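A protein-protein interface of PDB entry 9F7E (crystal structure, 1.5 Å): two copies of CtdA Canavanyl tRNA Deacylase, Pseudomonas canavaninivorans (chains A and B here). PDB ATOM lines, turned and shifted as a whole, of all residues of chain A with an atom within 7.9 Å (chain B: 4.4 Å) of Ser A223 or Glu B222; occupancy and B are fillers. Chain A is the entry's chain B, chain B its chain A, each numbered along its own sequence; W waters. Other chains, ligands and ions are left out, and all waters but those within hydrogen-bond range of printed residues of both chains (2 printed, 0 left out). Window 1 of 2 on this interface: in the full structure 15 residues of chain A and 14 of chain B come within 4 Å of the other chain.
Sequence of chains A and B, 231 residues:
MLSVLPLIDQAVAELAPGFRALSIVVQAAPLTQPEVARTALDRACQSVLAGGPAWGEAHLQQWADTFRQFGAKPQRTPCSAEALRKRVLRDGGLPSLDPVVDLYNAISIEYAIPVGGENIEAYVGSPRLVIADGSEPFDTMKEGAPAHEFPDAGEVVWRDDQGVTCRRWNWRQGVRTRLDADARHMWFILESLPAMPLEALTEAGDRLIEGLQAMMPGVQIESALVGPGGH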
ATOM      1  N   VAL A   4       7.409  17.137  -3.212  1.00  0.00           N
ATOM      2  CA  VAL A   4       7.332  18.228  -4.175  1.00  0.00           C
ATOM      3  C   VAL A   4       5.969  18.139  -4.834  1.00  0.00           C
ATOM      4  O   VAL A   4       5.572  17.067  -5.297  1.00  0.00           O
ATOM      5  CB  VAL A   4       8.439  18.166  -5.242  1.00  0.00           C
ATOM      6  CG1 VAL A   4       8.106  19.086  -6.412  1.00  0.00           C
ATOM      7  CG2 VAL A   4       9.772  18.575  -4.654  1.00  0.00           C
ATOM      8  N   ALA A  21       3.828  15.127 -17.483  1.00  0.00           N
ATOM      9  CA  ALA A  21       5.177  14.983 -16.978  1.00  0.00           C
ATOM     10  C   ALA A  21       5.229  13.951 -15.866  1.00  0.00           C
ATOM     11  O   ALA A  21       4.272  13.761 -15.125  1.00  0.00           O
ATOM     12  CB  ALA A  21       5.699  16.327 -16.476  1.00  0.00           C
ATOM     13  N   LEU A  22       6.370  13.317 -15.744  1.00  0.00           N
ATOM     14  CA  LEU A  22       6.667  12.527 -14.548  1.00  0.00           C
ATOM     15  C   LEU A  22       7.521  13.384 -13.622  1.00  0.00           C
ATOM     16  O   LEU A  22       8.617  13.810 -14.000  1.00  0.00           O
ATOM     17  CB  LEU A  22       7.400  11.239 -14.875  1.00  0.00           C
ATOM     18  CG  LEU A  22       6.562  10.024 -15.246  1.00  0.00           C
ATOM     19  CD1 LEU A  22       7.536   8.930 -15.686  1.00  0.00           C
ATOM     20  CD2 LEU A  22       5.688   9.588 -14.095  1.00  0.00           C
ATOM     21  N   SER A  23       7.047  13.562 -12.404  1.00  0.00           N
ATOM     22  CA  SER A  23       7.727  14.281 -11.343  1.00  0.00           C
ATOM     23  C   SER A  23       8.245  13.227 -10.371  1.00  0.00           C
ATOM     24  O   SER A  23       7.447  12.556  -9.718  1.00  0.00           O
ATOM     25  CB  SER A  23       6.727  15.214 -10.669  1.00  0.00           C
ATOM     26  OG  SER A  23       7.296  15.901  -9.587  1.00  0.00           O
ATOM     27  N   ILE A  24       9.567  13.076 -10.276  1.00  0.00           N
ATOM     28  CA  ILE A  24      10.220  12.026  -9.504  1.00  0.00           C
ATOM     29  C   ILE A  24      11.042  12.718  -8.433  1.00  0.00           C
ATOM     30  O   ILE A  24      11.963  13.483  -8.749  1.00  0.00           O
ATOM     31  CB  ILE A  24      11.113  11.140 -10.394  1.00  0.00           C
ATOM     32  CG1 ILE A  24      10.295  10.521 -11.543  1.00  0.00           C
ATOM     33  CG2 ILE A  24      11.805  10.058  -9.582  1.00  0.00           C
ATOM     34  CD1 ILE A  24      11.125   9.687 -12.547  1.00  0.00           C
ATOM     35  N   VAL A  25      10.705  12.444  -7.175  1.00  0.00           N
ATOM     36  CA  VAL A  25      11.382  13.015  -6.021  1.00  0.00           C
ATOM     37  C   VAL A  25      12.219  11.912  -5.376  1.00  0.00           C
ATOM     38  O   VAL A  25      11.742  10.789  -5.160  1.00  0.00           O
ATOM     39  CB  VAL A  25      10.392  13.625  -5.012  1.00  0.00           C
ATOM     40  CG1 VAL A  25      11.147  14.202  -3.800  1.00  0.00           C
ATOM     41  CG2 VAL A  25       9.569  14.695  -5.692  1.00  0.00           C
ATOM     42  N   VAL A  26      13.475  12.224  -5.121  1.00  0.00           N
ATOM     43  CA  VAL A  26      14.469  11.225  -4.772  1.00  0.00           C
ATOM     44  C   VAL A  26      15.164  11.664  -3.499  1.00  0.00           C
ATOM     45  O   VAL A  26      15.628  12.808  -3.388  1.00  0.00           O
ATOM     46  CB  VAL A  26      15.483  11.042  -5.914  1.00  0.00           C
ATOM     47  CG1 VAL A  26      16.553  10.083  -5.524  1.00  0.00           C
ATOM     48  CG2 VAL A  26      14.779  10.552  -7.191  1.00  0.00           C
ATOM     49  N   PHE A 188      13.457  15.309 -10.281  1.00  0.00           N
ATOM     50  CA  PHE A 188      13.590  15.127 -11.724  1.00  0.00           C
ATOM     51  C   PHE A 188      12.229  15.340 -12.374  1.00  0.00           C
ATOM     52  O   PHE A 188      11.224  14.815 -11.893  1.00  0.00           O
ATOM     53  CB  PHE A 188      14.113  13.731 -12.060  1.00  0.00           C
ATOM     54  CG  PHE A 188      15.436  13.426 -11.433  1.00  0.00           C
ATOM     55  CD1 PHE A 188      16.583  13.875 -12.033  1.00  0.00           C
ATOM     56  CD2 PHE A 188      15.532  12.705 -10.245  1.00  0.00           C
ATOM     57  CE1 PHE A 188      17.818  13.641 -11.481  1.00  0.00           C
ATOM     58  CE2 PHE A 188      16.779  12.473  -9.660  1.00  0.00           C
ATOM     59  CZ  PHE A 188      17.927  12.940 -10.274  1.00  0.00           C
ATOM     60  N   THR A 202       6.539   6.448 -19.476  1.00  0.00           N
ATOM     61  CA  THR A 202       6.669   5.477 -18.391  1.00  0.00           C
ATOM     62  C   THR A 202       8.000   4.756 -18.445  1.00  0.00           C
ATOM     63  O   THR A 202       8.672   4.567 -17.411  1.00  0.00           O
ATOM     64  CB  THR A 202       5.516   4.457 -18.516  1.00  0.00           C
ATOM     65  OG1 THR A 202       4.288   5.101 -18.154  1.00  0.00           O
ATOM     66  CG2 THR A 202       5.775   3.226 -17.706  1.00  0.00           C
ATOM     67  N   GLY A 205      10.868   6.984 -17.384  1.00  0.00           N
ATOM     68  CA  GLY A 205      10.901   7.122 -15.947  1.00  0.00           C
ATOM     69  C   GLY A 205      11.387   5.856 -15.267  1.00  0.00           C
ATOM     70  O   GLY A 205      12.171   5.920 -14.312  1.00  0.00           O
ATOM     71  N   ASP A 206      10.909   4.689 -15.723  1.00  0.00           N
ATOM     72  CA  ASP A 206      11.366   3.447 -15.116  1.00  0.00           C
ATOM     73  C   ASP A 206      12.856   3.262 -15.334  1.00  0.00           C
ATOM     74  O   ASP A 206      13.560   2.744 -14.467  1.00  0.00           O
ATOM     75  CB  ASP A 206      10.635   2.255 -15.704  1.00  0.00           C
ATOM     76  CG  ASP A 206       9.184   2.157 -15.257  1.00  0.00           C
ATOM     77  OD1 ASP A 206       8.821   2.779 -14.235  1.00  0.00           O
ATOM     78  OD2 ASP A 206       8.397   1.471 -15.967  1.00  0.00           O
ATOM     79  N   ILE A 209      14.716   5.527 -12.837  1.00  0.00           N
ATOM     80  CA  ILE A 209      14.650   5.016 -11.467  1.00  0.00           C
ATOM     81  C   ILE A 209      15.530   3.783 -11.299  1.00  0.00           C
ATOM     82  O   ILE A 209      16.245   3.642 -10.288  1.00  0.00           O
ATOM     83  CB  ILE A 209      13.183   4.723 -11.101  1.00  0.00           C
ATOM     84  CG1 ILE A 209      12.406   6.029 -10.905  1.00  0.00           C
ATOM     85  CG2 ILE A 209      13.072   3.844  -9.854  1.00  0.00           C
ATOM     86  CD1 ILE A 209      10.905   5.807 -10.823  1.00  0.00           C
ATOM     87  N   GLN A 220      15.451   6.208  -2.081  1.00  0.00           N
ATOM     88  CA  GLN A 220      14.010   6.168  -1.876  1.00  0.00           C
ATOM     89  C   GLN A 220      13.346   7.114  -2.868  1.00  0.00           C
ATOM     90  O   GLN A 220      13.867   8.205  -3.132  1.00  0.00           O
ATOM     91  CB  GLN A 220      13.607   6.545  -0.460  1.00  0.00           C
ATOM     92  CG  GLN A 220      12.119   6.411  -0.238  1.00  0.00           C
ATOM     93  CD  GLN A 220      11.747   6.655   1.197  1.00  0.00           C
ATOM     94  OE1 GLN A 220      12.623   6.814   2.052  1.00  0.00           O
ATOM     95  NE2 GLN A 220      10.450   6.628   1.488  1.00  0.00           N
ATOM     96  N   ILE A 221      12.214   6.687  -3.440  1.00  0.00           N
ATOM     97  CA  ILE A 221      11.616   7.352  -4.597  1.00  0.00           C
ATOM     98  C   ILE A 221      10.121   7.514  -4.400  1.00  0.00           C
ATOM     99  O   ILE A 221       9.438   6.581  -3.971  1.00  0.00           O
ATOM    100  CB  ILE A 221      11.922   6.540  -5.879  1.00  0.00           C
ATOM    101  CG1 ILE A 221      13.444   6.468  -6.024  1.00  0.00           C
ATOM    102  CG2 ILE A 221      11.235   7.136  -7.088  1.00  0.00           C
ATOM    103  CD1 ILE A 221      13.905   5.483  -7.045  1.00  0.00           C
ATOM    104  N   GLU A 222       9.617   8.701  -4.752  1.00  0.00           N
ATOM    105  CA  GLU A 222       8.185   8.981  -4.831  1.00  0.00           C
ATOM    106  C   GLU A 222       7.932   9.755  -6.120  1.00  0.00           C
ATOM    107  O   GLU A 222       8.513  10.819  -6.346  1.00  0.00           O
ATOM    108  CB  GLU A 222       7.696   9.770  -3.613  1.00  0.00           C
ATOM    109  CG  GLU A 222       6.200  10.057  -3.581  1.00  0.00           C
ATOM    110  CD  GLU A 222       5.769  10.914  -2.374  1.00  0.00           C
ATOM    111  OE1 GLU A 222       6.513  10.963  -1.358  1.00  0.00           O
ATOM    112  OE2 GLU A 222       4.683  11.538  -2.450  1.00  0.00           O
ATOM    113  N   SER A 223       7.092   9.213  -6.993  1.00  0.00           N
ATOM    114  CA  SER A 223       6.870   9.855  -8.281  1.00  0.00           C
ATOM    115  C   SER A 223       5.389  10.146  -8.508  1.00  0.00           C
ATOM    116  O   SER A 223       4.506   9.526  -7.921  1.00  0.00           O
ATOM    117  CB  SER A 223       7.437   9.011  -9.424  1.00  0.00           C
ATOM    118  OG  SER A 223       6.775   7.782  -9.500  1.00  0.00           O
ATOM    119  N   ALA A 224       5.124  11.134  -9.356  1.00  0.00           N
ATOM    120  CA  ALA A 224       3.755  11.516  -9.677  1.00  0.00           C
ATOM    121  C   ALA A 224       3.660  11.848 -11.154  1.00  0.00           C
ATOM    122  O   ALA A 224       4.568  12.452 -11.723  1.00  0.00           O
ATOM    123  CB  ALA A 224       3.287  12.716  -8.833  1.00  0.00           C
ATOM    124  N   LEU A 225       2.554  11.455 -11.777  1.00  0.00           N
ATOM    125  CA  LEU A 225       2.243  11.870 -13.143  1.00  0.00           C
ATOM    126  C   LEU A 225       1.385  13.123 -13.029  1.00  0.00           C
ATOM    127  O   LEU A 225       0.349  13.114 -12.338  1.00  0.00           O
ATOM    128  CB  LEU A 225       1.515  10.738 -13.861  1.00  0.00           C
ATOM    129  CG  LEU A 225       1.273  10.881 -15.357  1.00  0.00           C
ATOM    130  CD1 LEU A 225       2.571  10.726 -16.144  1.00  0.00           C
ATOM    131  CD2 LEU A 225       0.218   9.858 -15.795  1.00  0.00           C
ATOM    132  N   VAL A 226       1.833  14.210 -13.651  1.00  0.00           N
ATOM    133  CA  VAL A 226       1.171  15.497 -13.538  1.00  0.00           C
ATOM    134  C   VAL A 226       0.945  16.117 -14.920  1.00  0.00           C
ATOM    135  O   VAL A 226       1.574  15.746 -15.922  1.00  0.00           O
ATOM    136  CB  VAL A 226       1.992  16.453 -12.639  1.00  0.00           C
ATOM    137  CG1 VAL A 226       2.257  15.817 -11.283  1.00  0.00           C
ATOM    138  CG2 VAL A 226       3.287  16.838 -13.309  1.00  0.00           C
ATOM    139  N   MET B   1       3.173  -2.355 -11.623  1.00  0.00           N
ATOM    140  CA  MET B   1       4.024  -1.756 -10.552  1.00  0.00           C
ATOM    141  C   MET B   1       5.034  -0.806 -11.165  1.00  0.00           C
ATOM    142  O   MET B   1       5.235   0.307 -10.679  1.00  0.00           O
ATOM    143  CB  MET B   1       4.736  -2.838  -9.752  1.00  0.00           C
ATOM    144  CG  MET B   1       4.000  -3.195  -8.485  1.00  0.00           C
ATOM    145  SD  MET B   1       4.642  -2.439  -6.966  1.00  0.00           S
ATOM    146  CE  MET B   1       5.304  -0.869  -7.538  1.00  0.00           C
ATOM    147  N   LEU B   2       5.677  -1.253 -12.240  1.00  0.00           N
ATOM    148  CA  LEU B   2       6.499  -0.331 -13.005  1.00  0.00           C
ATOM    149  C   LEU B   2       5.654   0.731 -13.687  1.00  0.00           C
ATOM    150  O   LEU B   2       6.200   1.761 -14.106  1.00  0.00           O
ATOM    151  CB  LEU B   2       7.333  -1.096 -14.030  1.00  0.00           C
ATOM    152  CG  LEU B   2       8.757  -1.400 -13.550  1.00  0.00           C
ATOM    153  CD1 LEU B   2       8.789  -2.514 -12.512  1.00  0.00           C
ATOM    154  CD2 LEU B   2       9.641  -1.737 -14.752  1.00  0.00           C
ATOM    155  N   SER B   3       4.336   0.522 -13.761  1.00  0.00           N
ATOM    156  CA  SER B   3       3.434   1.530 -14.292  1.00  0.00           C
ATOM    157  C   SER B   3       1.980   1.086 -14.324  1.00  0.00           C
ATOM    158  O   SER B   3       1.401   0.946 -15.407  1.00  0.00           O
ATOM    159  CB  SER B   3       3.845   1.914 -15.711  1.00  0.00           C
ATOM    160  OG  SER B   3       2.924   2.830 -16.272  1.00  0.00           O
ATOM    161  N   VAL B   4       1.366   0.882 -13.160  1.00  0.00           N
ATOM    162  CA  VAL B   4      -0.063   0.596 -13.148  1.00  0.00           C
ATOM    163  C   VAL B   4      -0.804   1.886 -13.479  1.00  0.00           C
ATOM    164  O   VAL B   4      -0.634   2.906 -12.803  1.00  0.00           O
ATOM    165  CB  VAL B   4      -0.500   0.029 -11.793  1.00  0.00           C
ATOM    166  CG1 VAL B   4      -2.018   0.015 -11.689  1.00  0.00           C
ATOM    167  CG2 VAL B   4       0.097  -1.363 -11.593  1.00  0.00           C
ATOM    168  N   SER B  23      -4.733   7.310  -7.847  1.00  0.00           N
ATOM    169  CA  SER B  23      -4.259   5.957  -8.045  1.00  0.00           C
ATOM    170  C   SER B  23      -2.838   5.902  -7.510  1.00  0.00           C
ATOM    171  O   SER B  23      -1.967   6.629  -7.988  1.00  0.00           O
ATOM    172  CB  SER B  23      -4.330   5.601  -9.526  1.00  0.00           C
ATOM    173  OG  SER B  23      -3.842   4.312  -9.749  1.00  0.00           O
ATOM    174  N   ILE B  24      -2.640   5.136  -6.447  1.00  0.00           N
ATOM    175  CA  ILE B  24      -1.362   5.082  -5.740  1.00  0.00           C
ATOM    176  C   ILE B  24      -0.880   3.642  -5.786  1.00  0.00           C
ATOM    177  O   ILE B  24      -1.554   2.741  -5.289  1.00  0.00           O
ATOM    178  CB  ILE B  24      -1.497   5.609  -4.294  1.00  0.00           C
ATOM    179  CG1 ILE B  24      -1.993   7.056  -4.307  1.00  0.00           C
ATOM    180  CG2 ILE B  24      -0.169   5.518  -3.524  1.00  0.00           C
ATOM    181  CD1 ILE B  24      -2.294   7.659  -2.937  1.00  0.00           C
ATOM    182  N   VAL B  25       0.301   3.433  -6.370  1.00  0.00           N
ATOM    183  CA  VAL B  25       0.928   2.131  -6.525  1.00  0.00           C
ATOM    184  C   VAL B  25       2.161   2.100  -5.631  1.00  0.00           C
ATOM    185  O   VAL B  25       2.972   3.032  -5.656  1.00  0.00           O
ATOM    186  CB  VAL B  25       1.312   1.877  -7.990  1.00  0.00           C
ATOM    187  CG1 VAL B  25       1.988   0.536  -8.125  1.00  0.00           C
ATOM    188  CG2 VAL B  25       0.069   1.935  -8.873  1.00  0.00           C
ATOM    189  N   ILE B 221       6.807   4.662  -4.112  1.00  0.00           N
ATOM    190  CA  ILE B 221       5.429   5.085  -4.361  1.00  0.00           C
ATOM    191  C   ILE B 221       5.328   5.826  -5.682  1.00  0.00           C
ATOM    192  O   ILE B 221       6.186   6.640  -6.016  1.00  0.00           O
ATOM    193  CB  ILE B 221       4.886   5.985  -3.222  1.00  0.00           C
ATOM    194  CG1 ILE B 221       4.921   5.193  -1.904  1.00  0.00           C
ATOM    195  CG2 ILE B 221       3.514   6.483  -3.576  1.00  0.00           C
ATOM    196  CD1 ILE B 221       4.659   6.023  -0.693  1.00  0.00           C
ATOM    197  N   GLU B 222       4.264   5.555  -6.427  1.00  0.00           N
ATOM    198  CA  GLU B 222       3.943   6.319  -7.628  1.00  0.00           C
ATOM    199  C   GLU B 222       2.452   6.631  -7.616  1.00  0.00           C
ATOM    200  O   GLU B 222       1.628   5.790  -7.241  1.00  0.00           O
ATOM    201  CB  GLU B 222       4.367   5.581  -8.880  1.00  0.00           C
ATOM    202  CG  GLU B 222       3.875   4.188  -9.025  1.00  0.00           C
ATOM    203  CD  GLU B 222       4.558   3.461 -10.175  1.00  0.00           C
ATOM    204  OE1 GLU B 222       5.799   3.591 -10.321  1.00  0.00           O
ATOM    205  OE2 GLU B 222       3.849   2.770 -10.937  1.00  0.00           O
ATOM    206  N   SER B 223       2.116   7.860  -7.995  1.00  0.00           N
ATOM    207  CA  SER B 223       0.747   8.341  -7.919  1.00  0.00           C
ATOM    208  C   SER B 223       0.331   8.974  -9.233  1.00  0.00           C
ATOM    209  O   SER B 223       1.164   9.428 -10.011  1.00  0.00           O
ATOM    210  CB  SER B 223       0.577   9.373  -6.797  1.00  0.00           C
ATOM    211  OG  SER B 223       0.744   8.765  -5.536  1.00  0.00           O
HETATM  212  O   HOH W   1       3.542   9.848  -5.607  1.00  0.00           O
HETATM  213  O   HOH W   2       8.284   5.859  -7.965  1.00  0.00           O
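Among the printed residues, pairs that only touch across the chains: Ser A223 with Glu B222, Glu A222 with Ile B221, Ala A224 with Ser B223 and Thr A202 with Leu B2.
OG1 of Thr A202 sits close to OG of Ser B3 (3.2 Å).
O of Ile B221 is in hydrogen-bond range of N of Ser A223 (2.9 Å).
N of Ile B221 sits at hydrogen-bond distance from O of Ile A221, at 3.3 Å.
The side-chain carboxylate of Asp A206 sits close to the backbone carbonyl oxygen of Leu B2, at 2.8 Å.
The backbone carbonyl oxygen (O) of Ser A223 sits at hydrogen-bond distance from the backbone NH (N) of Ser B223, at 2.9 Å.
The backbone NH of Leu A225 lies within hydrogen-bond range of the backbone carbonyl oxygen of Ser B223, 3.0 Å away.
Ile A221 touches its own counterpart, Ile B221.
Glu A222 touches Ile B221, but with the chains exchanged Ile A221 does not touch Glu B222 (5.8 Å).
Ser A223 touches Ile B221, but with the chains exchanged Ile A221 does not touch Ser B223 (8.5 Å).
Ser A223 touches its own counterpart, Ser B223.
Of the 10 pairs that touch across the chains among the printed residues, 2 have their exchanged pair printed and touching as well.
Val A25 touches none of the printed residues of chain B.
Phe A188 touches none of the printed residues of chain B.
Printed residues of chain B within 4 Å of Leu A225: Ser B223 (3.0 Å).
Of the printed residues of chain A, Ser B3 touches Thr A202.
Glu B222 touches just one residue of chain A: Ser A223.
Of the printed residues of chain A, Ser B223 touches Ser A223, Ala A224 and Leu A225.
The nearest printed residue of chain B that does not touch Ser A223 is Val B25 (7.0 Å).
The nearest printed residue of chain A that does not touch Ser B3 is Asp A206 (4.6 Å).
Of the 10 printed residues of chain B, 5 touch a printed residue of chain A.
Printed residues of chain B that touch a printed residue of chain A: Leu B2, Ser B3, Ile B221, Glu B222 and Ser B223.
Among the printed residues, 10 pairs touch across the chains.
Among the printed residues, no Asp or Glu carboxylate lies within 4 Å of a Lys or Arg side-chain nitrogen of the other chain.
The backbone NH (N) of Val A25 sits at hydrogen-bond distance from the backbone carbonyl oxygen (O) of Glu A222.
N of Ala A224 lies within hydrogen-bond range of O of Ser A23.
The backbone NH (N) of Val B25 lies within hydrogen-bond range of the backbone carbonyl oxygen (O) of Glu B222, 2.8 Å away.
Water W1 bridges O of Ser A223 and OG of Ser B223.
Water W2 lies within hydrogen-bond range of OG of Ser A223 (2.9 Å) and O of Ile B221 (3.0 Å).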
